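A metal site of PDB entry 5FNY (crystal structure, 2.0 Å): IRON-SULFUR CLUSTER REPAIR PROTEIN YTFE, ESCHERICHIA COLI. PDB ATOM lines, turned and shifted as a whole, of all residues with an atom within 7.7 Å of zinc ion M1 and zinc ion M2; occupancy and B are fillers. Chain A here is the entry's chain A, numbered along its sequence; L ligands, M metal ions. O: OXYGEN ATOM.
The backbone NH of Phe 213 lies within hydrogen-bond range of the backbone carbonyl oxygen of Glu 208 (2.9 Å).
The backbone carbonyl oxygen (O) of Glu 133 is in hydrogen-bond range of the backbone NH (N) of Phe 138.
A ring nitrogen (ND1) of His 129 is in hydrogen-bond range of the side-chain carboxylate of Glu 159, at 2.7 Å.
The backbone NH of His 84 sits at hydrogen-bond distance from the backbone carbonyl oxygen of Ile 79 (2.9 Å).
OE2 of Glu 134 lies within hydrogen-bond range of ND1 of His 84, at 2.7 Å.
OD1 of Asn 209 sits at hydrogen-bond distance from ND1 of His 160 (2.8 Å).
NE2 of His 87 is in hydrogen-bond range of ND1 of His 204, 3.1 Å away.
Of the 23 residues printed, 4 come within 4 Å of zinc ion M1.
The nearest printed residue that does not touch zinc ion M1 is His 204 (4.3 Å).
Merely in contact with zinc ion M2: Ile 79.
Of the 23 residues printed, 5 come within 4 Å of zinc ion M2.
The nearest printed residue that does not touch zinc ion M2 is Phe 138 (4.3 Å).
Zinc ion M1 is bound by O of the ligand (1.9 Å), OE2 of Glu 133 (2.0 Å), NE2 of His 129 (2.1 Å), NE2 of His 160 (2.1 Å) and OE1 of Glu 208 (2.2 Å).
Zinc ion M1 has five donor atoms within binding distance.
Zinc ion M2 is bound by an oxygen (O) of the ligand (1.9 Å), the side-chain carboxylate of Glu 208 (2.0 Å), a ring nitrogen (NE2) of His 84 (2.1 Å), a ring nitrogen (NE2) of His 204 (2.1 Å) and the side-chain carboxylate of Glu 133 (2.2 Å).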
ATOM      1  N   ILE A  79     -29.340 -14.961 -33.672  1.00  0.00           N
ATOM      2  CA  ILE A  79     -29.319 -13.705 -32.925  1.00  0.00           C
ATOM      3  C   ILE A  79     -28.628 -12.605 -33.721  1.00  0.00           C
ATOM      4  O   ILE A  79     -29.165 -11.491 -33.844  1.00  0.00           O
ATOM      5  CB  ILE A  79     -28.668 -13.881 -31.558  1.00  0.00           C
ATOM      6  CG1 ILE A  79     -29.599 -14.677 -30.646  1.00  0.00           C
ATOM      7  CG2 ILE A  79     -28.326 -12.521 -30.923  1.00  0.00           C
ATOM      8  CD1 ILE A  79     -28.955 -15.183 -29.380  1.00  0.00           C
ATOM      9  N   ILE A  80     -27.458 -12.925 -34.270  1.00  0.00           N
ATOM     10  CA  ILE A  80     -26.650 -11.949 -34.994  1.00  0.00           C
ATOM     11  C   ILE A  80     -27.399 -11.405 -36.219  1.00  0.00           C
ATOM     12  O   ILE A  80     -27.460 -10.183 -36.404  1.00  0.00           O
ATOM     13  CB  ILE A  80     -25.269 -12.508 -35.373  1.00  0.00           C
ATOM     14  CG1 ILE A  80     -24.450 -12.765 -34.107  1.00  0.00           C
ATOM     15  CG2 ILE A  80     -24.526 -11.526 -36.259  1.00  0.00           C
ATOM     16  CD1 ILE A  80     -23.221 -13.610 -34.321  1.00  0.00           C
ATOM     17  N   TYR A  83     -31.572 -10.252 -35.022  1.00  0.00           N
ATOM     18  CA  TYR A  83     -31.656  -9.241 -33.991  1.00  0.00           C
ATOM     19  C   TYR A  83     -30.521  -8.202 -34.007  1.00  0.00           C
ATOM     20  O   TYR A  83     -30.807  -7.023 -34.253  1.00  0.00           O
ATOM     21  CB  TYR A  83     -31.822  -9.880 -32.621  1.00  0.00           C
ATOM     22  CG  TYR A  83     -33.116 -10.680 -32.526  1.00  0.00           C
ATOM     23  CD1 TYR A  83     -34.374 -10.068 -32.732  1.00  0.00           C
ATOM     24  CD2 TYR A  83     -33.105 -12.043 -32.254  1.00  0.00           C
ATOM     25  CE1 TYR A  83     -35.551 -10.771 -32.643  1.00  0.00           C
ATOM     26  CE2 TYR A  83     -34.296 -12.773 -32.172  1.00  0.00           C
ATOM     27  CZ  TYR A  83     -35.507 -12.133 -32.397  1.00  0.00           C
ATOM     28  OH  TYR A  83     -36.681 -12.859 -32.316  1.00  0.00           O
ATOM     29  N   HIS A  84     -29.267  -8.617 -33.803  1.00  0.00           N
ATOM     30  CA  HIS A  84     -28.153  -7.655 -33.738  1.00  0.00           C
ATOM     31  C   HIS A  84     -28.095  -6.749 -34.975  1.00  0.00           C
ATOM     32  O   HIS A  84     -28.113  -5.527 -34.865  1.00  0.00           O
ATOM     33  CB  HIS A  84     -26.789  -8.334 -33.538  1.00  0.00           C
ATOM     34  CG  HIS A  84     -26.592  -8.896 -32.159  1.00  0.00           C
ATOM     35  ND1 HIS A  84     -25.350  -9.184 -31.663  1.00  0.00           N
ATOM     36  CD2 HIS A  84     -27.460  -9.171 -31.163  1.00  0.00           C
ATOM     37  CE1 HIS A  84     -25.460  -9.638 -30.426  1.00  0.00           C
ATOM     38  NE2 HIS A  84     -26.729  -9.636 -30.083  1.00  0.00           N
ATOM     39  N   HIS A  87     -31.192  -4.418 -35.235  1.00  0.00           N
ATOM     40  CA  HIS A  87     -31.074  -3.231 -34.381  1.00  0.00           C
ATOM     41  C   HIS A  87     -30.133  -2.160 -34.940  1.00  0.00           C
ATOM     42  O   HIS A  87     -30.417  -0.988 -34.806  1.00  0.00           O
ATOM     43  CB  HIS A  87     -30.557  -3.597 -33.015  1.00  0.00           C
ATOM     44  CG  HIS A  87     -31.434  -4.538 -32.263  1.00  0.00           C
ATOM     45  ND1 HIS A  87     -32.793  -4.582 -32.449  1.00  0.00           N
ATOM     46  CD2 HIS A  87     -31.145  -5.438 -31.294  1.00  0.00           C
ATOM     47  CE1 HIS A  87     -33.306  -5.505 -31.655  1.00  0.00           C
ATOM     48  NE2 HIS A  87     -32.338  -6.036 -30.942  1.00  0.00           N
ATOM     49  N   LEU A 126     -26.244  -0.447 -26.818  1.00  0.00           N
ATOM     50  CA  LEU A 126     -26.422  -1.644 -27.622  1.00  0.00           C
ATOM     51  C   LEU A 126     -25.226  -1.963 -28.505  1.00  0.00           C
ATOM     52  O   LEU A 126     -24.831  -3.108 -28.577  1.00  0.00           O
ATOM     53  CB  LEU A 126     -27.682  -1.545 -28.509  1.00  0.00           C
ATOM     54  CG  LEU A 126     -29.001  -1.986 -27.894  1.00  0.00           C
ATOM     55  CD1 LEU A 126     -30.084  -1.857 -28.966  1.00  0.00           C
ATOM     56  CD2 LEU A 126     -28.915  -3.422 -27.393  1.00  0.00           C
ATOM     57  N   HIS A 129     -22.394  -3.350 -26.372  1.00  0.00           N
ATOM     58  CA  HIS A 129     -22.852  -4.649 -25.868  1.00  0.00           C
ATOM     59  C   HIS A 129     -22.784  -5.770 -26.926  1.00  0.00           C
ATOM     60  O   HIS A 129     -22.246  -6.852 -26.673  1.00  0.00           O
ATOM     61  CB  HIS A 129     -24.267  -4.512 -25.356  1.00  0.00           C
ATOM     62  CG  HIS A 129     -24.860  -5.795 -24.897  1.00  0.00           C
ATOM     63  ND1 HIS A 129     -24.666  -6.291 -23.630  1.00  0.00           N
ATOM     64  CD2 HIS A 129     -25.649  -6.676 -25.540  1.00  0.00           C
ATOM     65  CE1 HIS A 129     -25.314  -7.439 -23.517  1.00  0.00           C
ATOM     66  NE2 HIS A 129     -25.908  -7.701 -24.670  1.00  0.00           N
ATOM     67  N   MET A 130     -23.304  -5.480 -28.107  1.00  0.00           N
ATOM     68  CA  MET A 130     -23.361  -6.473 -29.167  1.00  0.00           C
ATOM     69  C   MET A 130     -21.964  -6.827 -29.682  1.00  0.00           C
ATOM     70  O   MET A 130     -21.726  -7.950 -30.124  1.00  0.00           O
ATOM     71  CB  MET A 130     -24.253  -5.990 -30.326  1.00  0.00           C
ATOM     72  CG  MET A 130     -25.715  -5.898 -29.958  1.00  0.00           C
ATOM     73  SD  MET A 130     -26.869  -5.390 -31.277  1.00  0.00           S
ATOM     74  CE  MET A 130     -26.146  -3.900 -31.947  1.00  0.00           C
ATOM     75  N   GLU A 133     -20.395  -9.338 -27.221  1.00  0.00           N
ATOM     76  CA  GLU A 133     -21.015 -10.632 -27.483  1.00  0.00           C
ATOM     77  C   GLU A 133     -20.384 -11.244 -28.706  1.00  0.00           C
ATOM     78  O   GLU A 133     -19.853 -12.345 -28.623  1.00  0.00           O
ATOM     79  CB  GLU A 133     -22.539 -10.544 -27.641  1.00  0.00           C
ATOM     80  CG  GLU A 133     -23.247 -10.589 -26.312  1.00  0.00           C
ATOM     81  CD  GLU A 133     -24.771 -10.383 -26.393  1.00  0.00           C
ATOM     82  OE1 GLU A 133     -25.316 -10.027 -27.473  1.00  0.00           O
ATOM     83  OE2 GLU A 133     -25.415 -10.520 -25.343  1.00  0.00           O
ATOM     84  N   GLU A 134     -20.424 -10.527 -29.829  1.00  0.00           N
ATOM     85  CA  GLU A 134     -19.993 -11.104 -31.120  1.00  0.00           C
ATOM     86  C   GLU A 134     -18.494 -11.425 -31.149  1.00  0.00           C
ATOM     87  O   GLU A 134     -18.099 -12.449 -31.669  1.00  0.00           O
ATOM     88  CB  GLU A 134     -20.376 -10.180 -32.287  1.00  0.00           C
ATOM     89  CG  GLU A 134     -21.878 -10.143 -32.548  1.00  0.00           C
ATOM     90  CD  GLU A 134     -22.316  -9.065 -33.544  1.00  0.00           C
ATOM     91  OE1 GLU A 134     -21.522  -8.641 -34.405  1.00  0.00           O
ATOM     92  OE2 GLU A 134     -23.497  -8.636 -33.482  1.00  0.00           O
ATOM     93  N   LEU A 137     -17.633 -13.155 -26.197  1.00  0.00           N
ATOM     94  CA  LEU A 137     -18.442 -14.140 -25.521  1.00  0.00           C
ATOM     95  C   LEU A 137     -19.050 -15.221 -26.442  1.00  0.00           C
ATOM     96  O   LEU A 137     -18.946 -16.420 -26.141  1.00  0.00           O
ATOM     97  CB  LEU A 137     -19.560 -13.458 -24.707  1.00  0.00           C
ATOM     98  CG  LEU A 137     -20.441 -14.387 -23.890  1.00  0.00           C
ATOM     99  CD1 LEU A 137     -19.644 -15.191 -22.886  1.00  0.00           C
ATOM    100  CD2 LEU A 137     -21.562 -13.614 -23.211  1.00  0.00           C
ATOM    101  N   PHE A 138     -19.673 -14.833 -27.539  1.00  0.00           N
ATOM    102  CA  PHE A 138     -20.304 -15.846 -28.426  1.00  0.00           C
ATOM    103  C   PHE A 138     -19.300 -16.892 -28.987  1.00  0.00           C
ATOM    104  O   PHE A 138     -19.615 -18.078 -29.049  1.00  0.00           O
ATOM    105  CB  PHE A 138     -21.096 -15.210 -29.585  1.00  0.00           C
ATOM    106  CG  PHE A 138     -22.408 -14.548 -29.203  1.00  0.00           C
ATOM    107  CD1 PHE A 138     -23.007 -14.693 -27.936  1.00  0.00           C
ATOM    108  CD2 PHE A 138     -23.113 -13.814 -30.175  1.00  0.00           C
ATOM    109  CE1 PHE A 138     -24.242 -14.101 -27.656  1.00  0.00           C
ATOM    110  CE2 PHE A 138     -24.339 -13.233 -29.884  1.00  0.00           C
ATOM    111  CZ  PHE A 138     -24.903 -13.381 -28.630  1.00  0.00           C
ATOM    112  N   MET A 156     -23.283  -9.564 -18.892  1.00  0.00           N
ATOM    113  CA  MET A 156     -24.163  -9.344 -20.020  1.00  0.00           C
ATOM    114  C   MET A 156     -25.634  -9.239 -19.571  1.00  0.00           C
ATOM    115  O   MET A 156     -26.395  -8.442 -20.117  1.00  0.00           O
ATOM    116  CB  MET A 156     -24.018 -10.459 -21.049  1.00  0.00           C
ATOM    117  CG  MET A 156     -22.640 -10.567 -21.674  1.00  0.00           C
ATOM    118  SD  MET A 156     -22.120  -9.120 -22.617  1.00  0.00           S
ATOM    119  CE  MET A 156     -21.176  -8.190 -21.429  1.00  0.00           C
ATOM    120  N   GLU A 157     -26.030 -10.035 -18.584  1.00  0.00           N
ATOM    121  CA  GLU A 157     -27.407  -9.948 -18.109  1.00  0.00           C
ATOM    122  C   GLU A 157     -27.658  -8.634 -17.383  1.00  0.00           C
ATOM    123  O   GLU A 157     -28.760  -8.084 -17.464  1.00  0.00           O
ATOM    124  CB  GLU A 157     -27.781 -11.178 -17.262  1.00  0.00           C
ATOM    125  CG  GLU A 157     -27.763 -12.449 -18.086  1.00  0.00           C
ATOM    126  CD  GLU A 157     -28.437 -13.642 -17.414  1.00  0.00           C
ATOM    127  OE1 GLU A 157     -28.508 -13.689 -16.167  1.00  0.00           O
ATOM    128  OE2 GLU A 157     -28.877 -14.565 -18.154  1.00  0.00           O
ATOM    129  N   GLU A 159     -26.196  -5.831 -18.280  1.00  0.00           N
ATOM    130  CA  GLU A 159     -26.352  -4.911 -19.410  1.00  0.00           C
ATOM    131  C   GLU A 159     -27.741  -5.019 -20.087  1.00  0.00           C
ATOM    132  O   GLU A 159     -28.323  -4.000 -20.468  1.00  0.00           O
ATOM    133  CB  GLU A 159     -25.216  -5.113 -20.419  1.00  0.00           C
ATOM    134  CG  GLU A 159     -23.852  -4.672 -19.853  1.00  0.00           C
ATOM    135  CD  GLU A 159     -22.709  -4.666 -20.861  1.00  0.00           C
ATOM    136  OE1 GLU A 159     -22.901  -5.036 -22.049  1.00  0.00           O
ATOM    137  OE2 GLU A 159     -21.584  -4.292 -20.468  1.00  0.00           O
ATOM    138  N   HIS A 160     -28.291  -6.224 -20.185  1.00  0.00           N
ATOM    139  CA  HIS A 160     -29.686  -6.375 -20.620  1.00  0.00           C
ATOM    140  C   HIS A 160     -30.677  -5.623 -19.732  1.00  0.00           C
ATOM    141  O   HIS A 160     -31.609  -4.965 -20.241  1.00  0.00           O
ATOM    142  CB  HIS A 160     -30.074  -7.850 -20.657  1.00  0.00           C
ATOM    143  CG  HIS A 160     -29.337  -8.618 -21.698  1.00  0.00           C
ATOM    144  ND1 HIS A 160     -29.349  -9.995 -21.743  1.00  0.00           N
ATOM    145  CD2 HIS A 160     -28.535  -8.221 -22.712  1.00  0.00           C
ATOM    146  CE1 HIS A 160     -28.628 -10.403 -22.767  1.00  0.00           C
ATOM    147  NE2 HIS A 160     -28.115  -9.354 -23.369  1.00  0.00           N
ATOM    148  N   LEU A 201     -36.318  -6.294 -29.347  1.00  0.00           N
ATOM    149  CA  LEU A 201     -35.350  -6.255 -28.272  1.00  0.00           C
ATOM    150  C   LEU A 201     -35.737  -7.209 -27.159  1.00  0.00           C
ATOM    151  O   LEU A 201     -34.867  -7.888 -26.581  1.00  0.00           O
ATOM    152  CB  LEU A 201     -35.176  -4.814 -27.798  1.00  0.00           C
ATOM    153  CG  LEU A 201     -33.958  -4.398 -27.020  1.00  0.00           C
ATOM    154  CD1 LEU A 201     -32.669  -5.060 -27.488  1.00  0.00           C
ATOM    155  CD2 LEU A 201     -33.857  -2.881 -27.105  1.00  0.00           C
ATOM    156  N   HIS A 204     -35.141 -10.774 -28.499  1.00  0.00           N
ATOM    157  CA  HIS A 204     -33.680 -10.929 -28.505  1.00  0.00           C
ATOM    158  C   HIS A 204     -33.167 -11.228 -27.094  1.00  0.00           C
ATOM    159  O   HIS A 204     -32.506 -12.255 -26.875  1.00  0.00           O
ATOM    160  CB  HIS A 204     -33.084  -9.646 -29.122  1.00  0.00           C
ATOM    161  CG  HIS A 204     -31.595  -9.463 -28.967  1.00  0.00           C
ATOM    162  ND1 HIS A 204     -31.011  -8.230 -29.178  1.00  0.00           N
ATOM    163  CD2 HIS A 204     -30.576 -10.303 -28.656  1.00  0.00           C
ATOM    164  CE1 HIS A 204     -29.720  -8.309 -28.950  1.00  0.00           C
ATOM    165  NE2 HIS A 204     -29.418  -9.556 -28.653  1.00  0.00           N
ATOM    166  N   ILE A 205     -33.491 -10.372 -26.151  1.00  0.00           N
ATOM    167  CA  ILE A 205     -33.004 -10.554 -24.787  1.00  0.00           C
ATOM    168  C   ILE A 205     -33.595 -11.844 -24.211  1.00  0.00           C
ATOM    169  O   ILE A 205     -32.905 -12.570 -23.452  1.00  0.00           O
ATOM    170  CB  ILE A 205     -33.334  -9.347 -23.885  1.00  0.00           C
ATOM    171  CG1 ILE A 205     -32.690  -8.029 -24.369  1.00  0.00           C
ATOM    172  CG2 ILE A 205     -33.037  -9.643 -22.415  1.00  0.00           C
ATOM    173  CD1 ILE A 205     -31.254  -8.118 -24.770  1.00  0.00           C
ATOM    174  N   GLU A 208     -31.584 -14.805 -25.343  1.00  0.00           N
ATOM    175  CA  GLU A 208     -30.298 -14.882 -24.640  1.00  0.00           C
ATOM    176  C   GLU A 208     -30.475 -15.314 -23.177  1.00  0.00           C
ATOM    177  O   GLU A 208     -29.846 -16.291 -22.743  1.00  0.00           O
ATOM    178  CB  GLU A 208     -29.537 -13.569 -24.780  1.00  0.00           C
ATOM    179  CG  GLU A 208     -29.127 -13.298 -26.222  1.00  0.00           C
ATOM    180  CD  GLU A 208     -28.326 -12.029 -26.442  1.00  0.00           C
ATOM    181  OE1 GLU A 208     -28.076 -11.298 -25.464  1.00  0.00           O
ATOM    182  OE2 GLU A 208     -27.906 -11.784 -27.608  1.00  0.00           O
ATOM    183  N   ASN A 209     -31.352 -14.627 -22.445  1.00  0.00           N
ATOM    184  CA  ASN A 209     -31.557 -14.863 -21.004  1.00  0.00           C
ATOM    185  C   ASN A 209     -32.250 -16.149 -20.638  1.00  0.00           C
ATOM    186  O   ASN A 209     -31.960 -16.727 -19.599  1.00  0.00           O
ATOM    187  CB  ASN A 209     -32.349 -13.726 -20.350  1.00  0.00           C
ATOM    188  CG  ASN A 209     -31.493 -12.491 -20.078  1.00  0.00           C
ATOM    189  OD1 ASN A 209     -30.375 -12.365 -20.547  1.00  0.00           O
ATOM    190  ND2 ASN A 209     -32.041 -11.576 -19.312  1.00  0.00           N
ATOM    191  N   LEU A 212     -30.066 -19.250 -24.415  1.00  0.00           N
ATOM    192  CA  LEU A 212     -28.647 -19.345 -24.710  1.00  0.00           C
ATOM    193  C   LEU A 212     -27.775 -19.387 -23.455  1.00  0.00           C
ATOM    194  O   LEU A 212     -26.971 -20.322 -23.299  1.00  0.00           O
ATOM    195  CB  LEU A 212     -28.183 -18.199 -25.597  1.00  0.00           C
ATOM    196  CG  LEU A 212     -26.718 -18.253 -26.073  1.00  0.00           C
ATOM    197  CD1 LEU A 212     -26.447 -19.433 -27.004  1.00  0.00           C
ATOM    198  CD2 LEU A 212     -26.332 -16.932 -26.725  1.00  0.00           C
ATOM    199  N   PHE A 213     -27.934 -18.409 -22.590  1.00  0.00           N
ATOM    200  CA  PHE A 213     -27.096 -18.332 -21.403  1.00  0.00           C
ATOM    201  C   PHE A 213     -27.314 -19.464 -20.408  1.00  0.00           C
ATOM    202  O   PHE A 213     -26.333 -20.023 -19.932  1.00  0.00           O
ATOM    203  CB  PHE A 213     -27.212 -16.987 -20.699  1.00  0.00           C
ATOM    204  CG  PHE A 213     -26.703 -15.811 -21.513  1.00  0.00           C
ATOM    205  CD1 PHE A 213     -25.884 -15.960 -22.637  1.00  0.00           C
ATOM    206  CD2 PHE A 213     -27.052 -14.522 -21.122  1.00  0.00           C
ATOM    207  CE1 PHE A 213     -25.449 -14.853 -23.344  1.00  0.00           C
ATOM    208  CE2 PHE A 213     -26.595 -13.430 -21.814  1.00  0.00           C
ATOM    209  CZ  PHE A 213     -25.816 -13.588 -22.943  1.00  0.00           C
HETATM  210  O     O L   1     -27.572  -8.702 -26.758  1.00  0.00           O
HETATM  211 ZN    ZN M   1     -26.998  -9.390 -25.101  1.00  0.00          ZN
HETATM  212 ZN    ZN M   2     -27.440  -9.969 -28.181  1.00  0.00          ZN
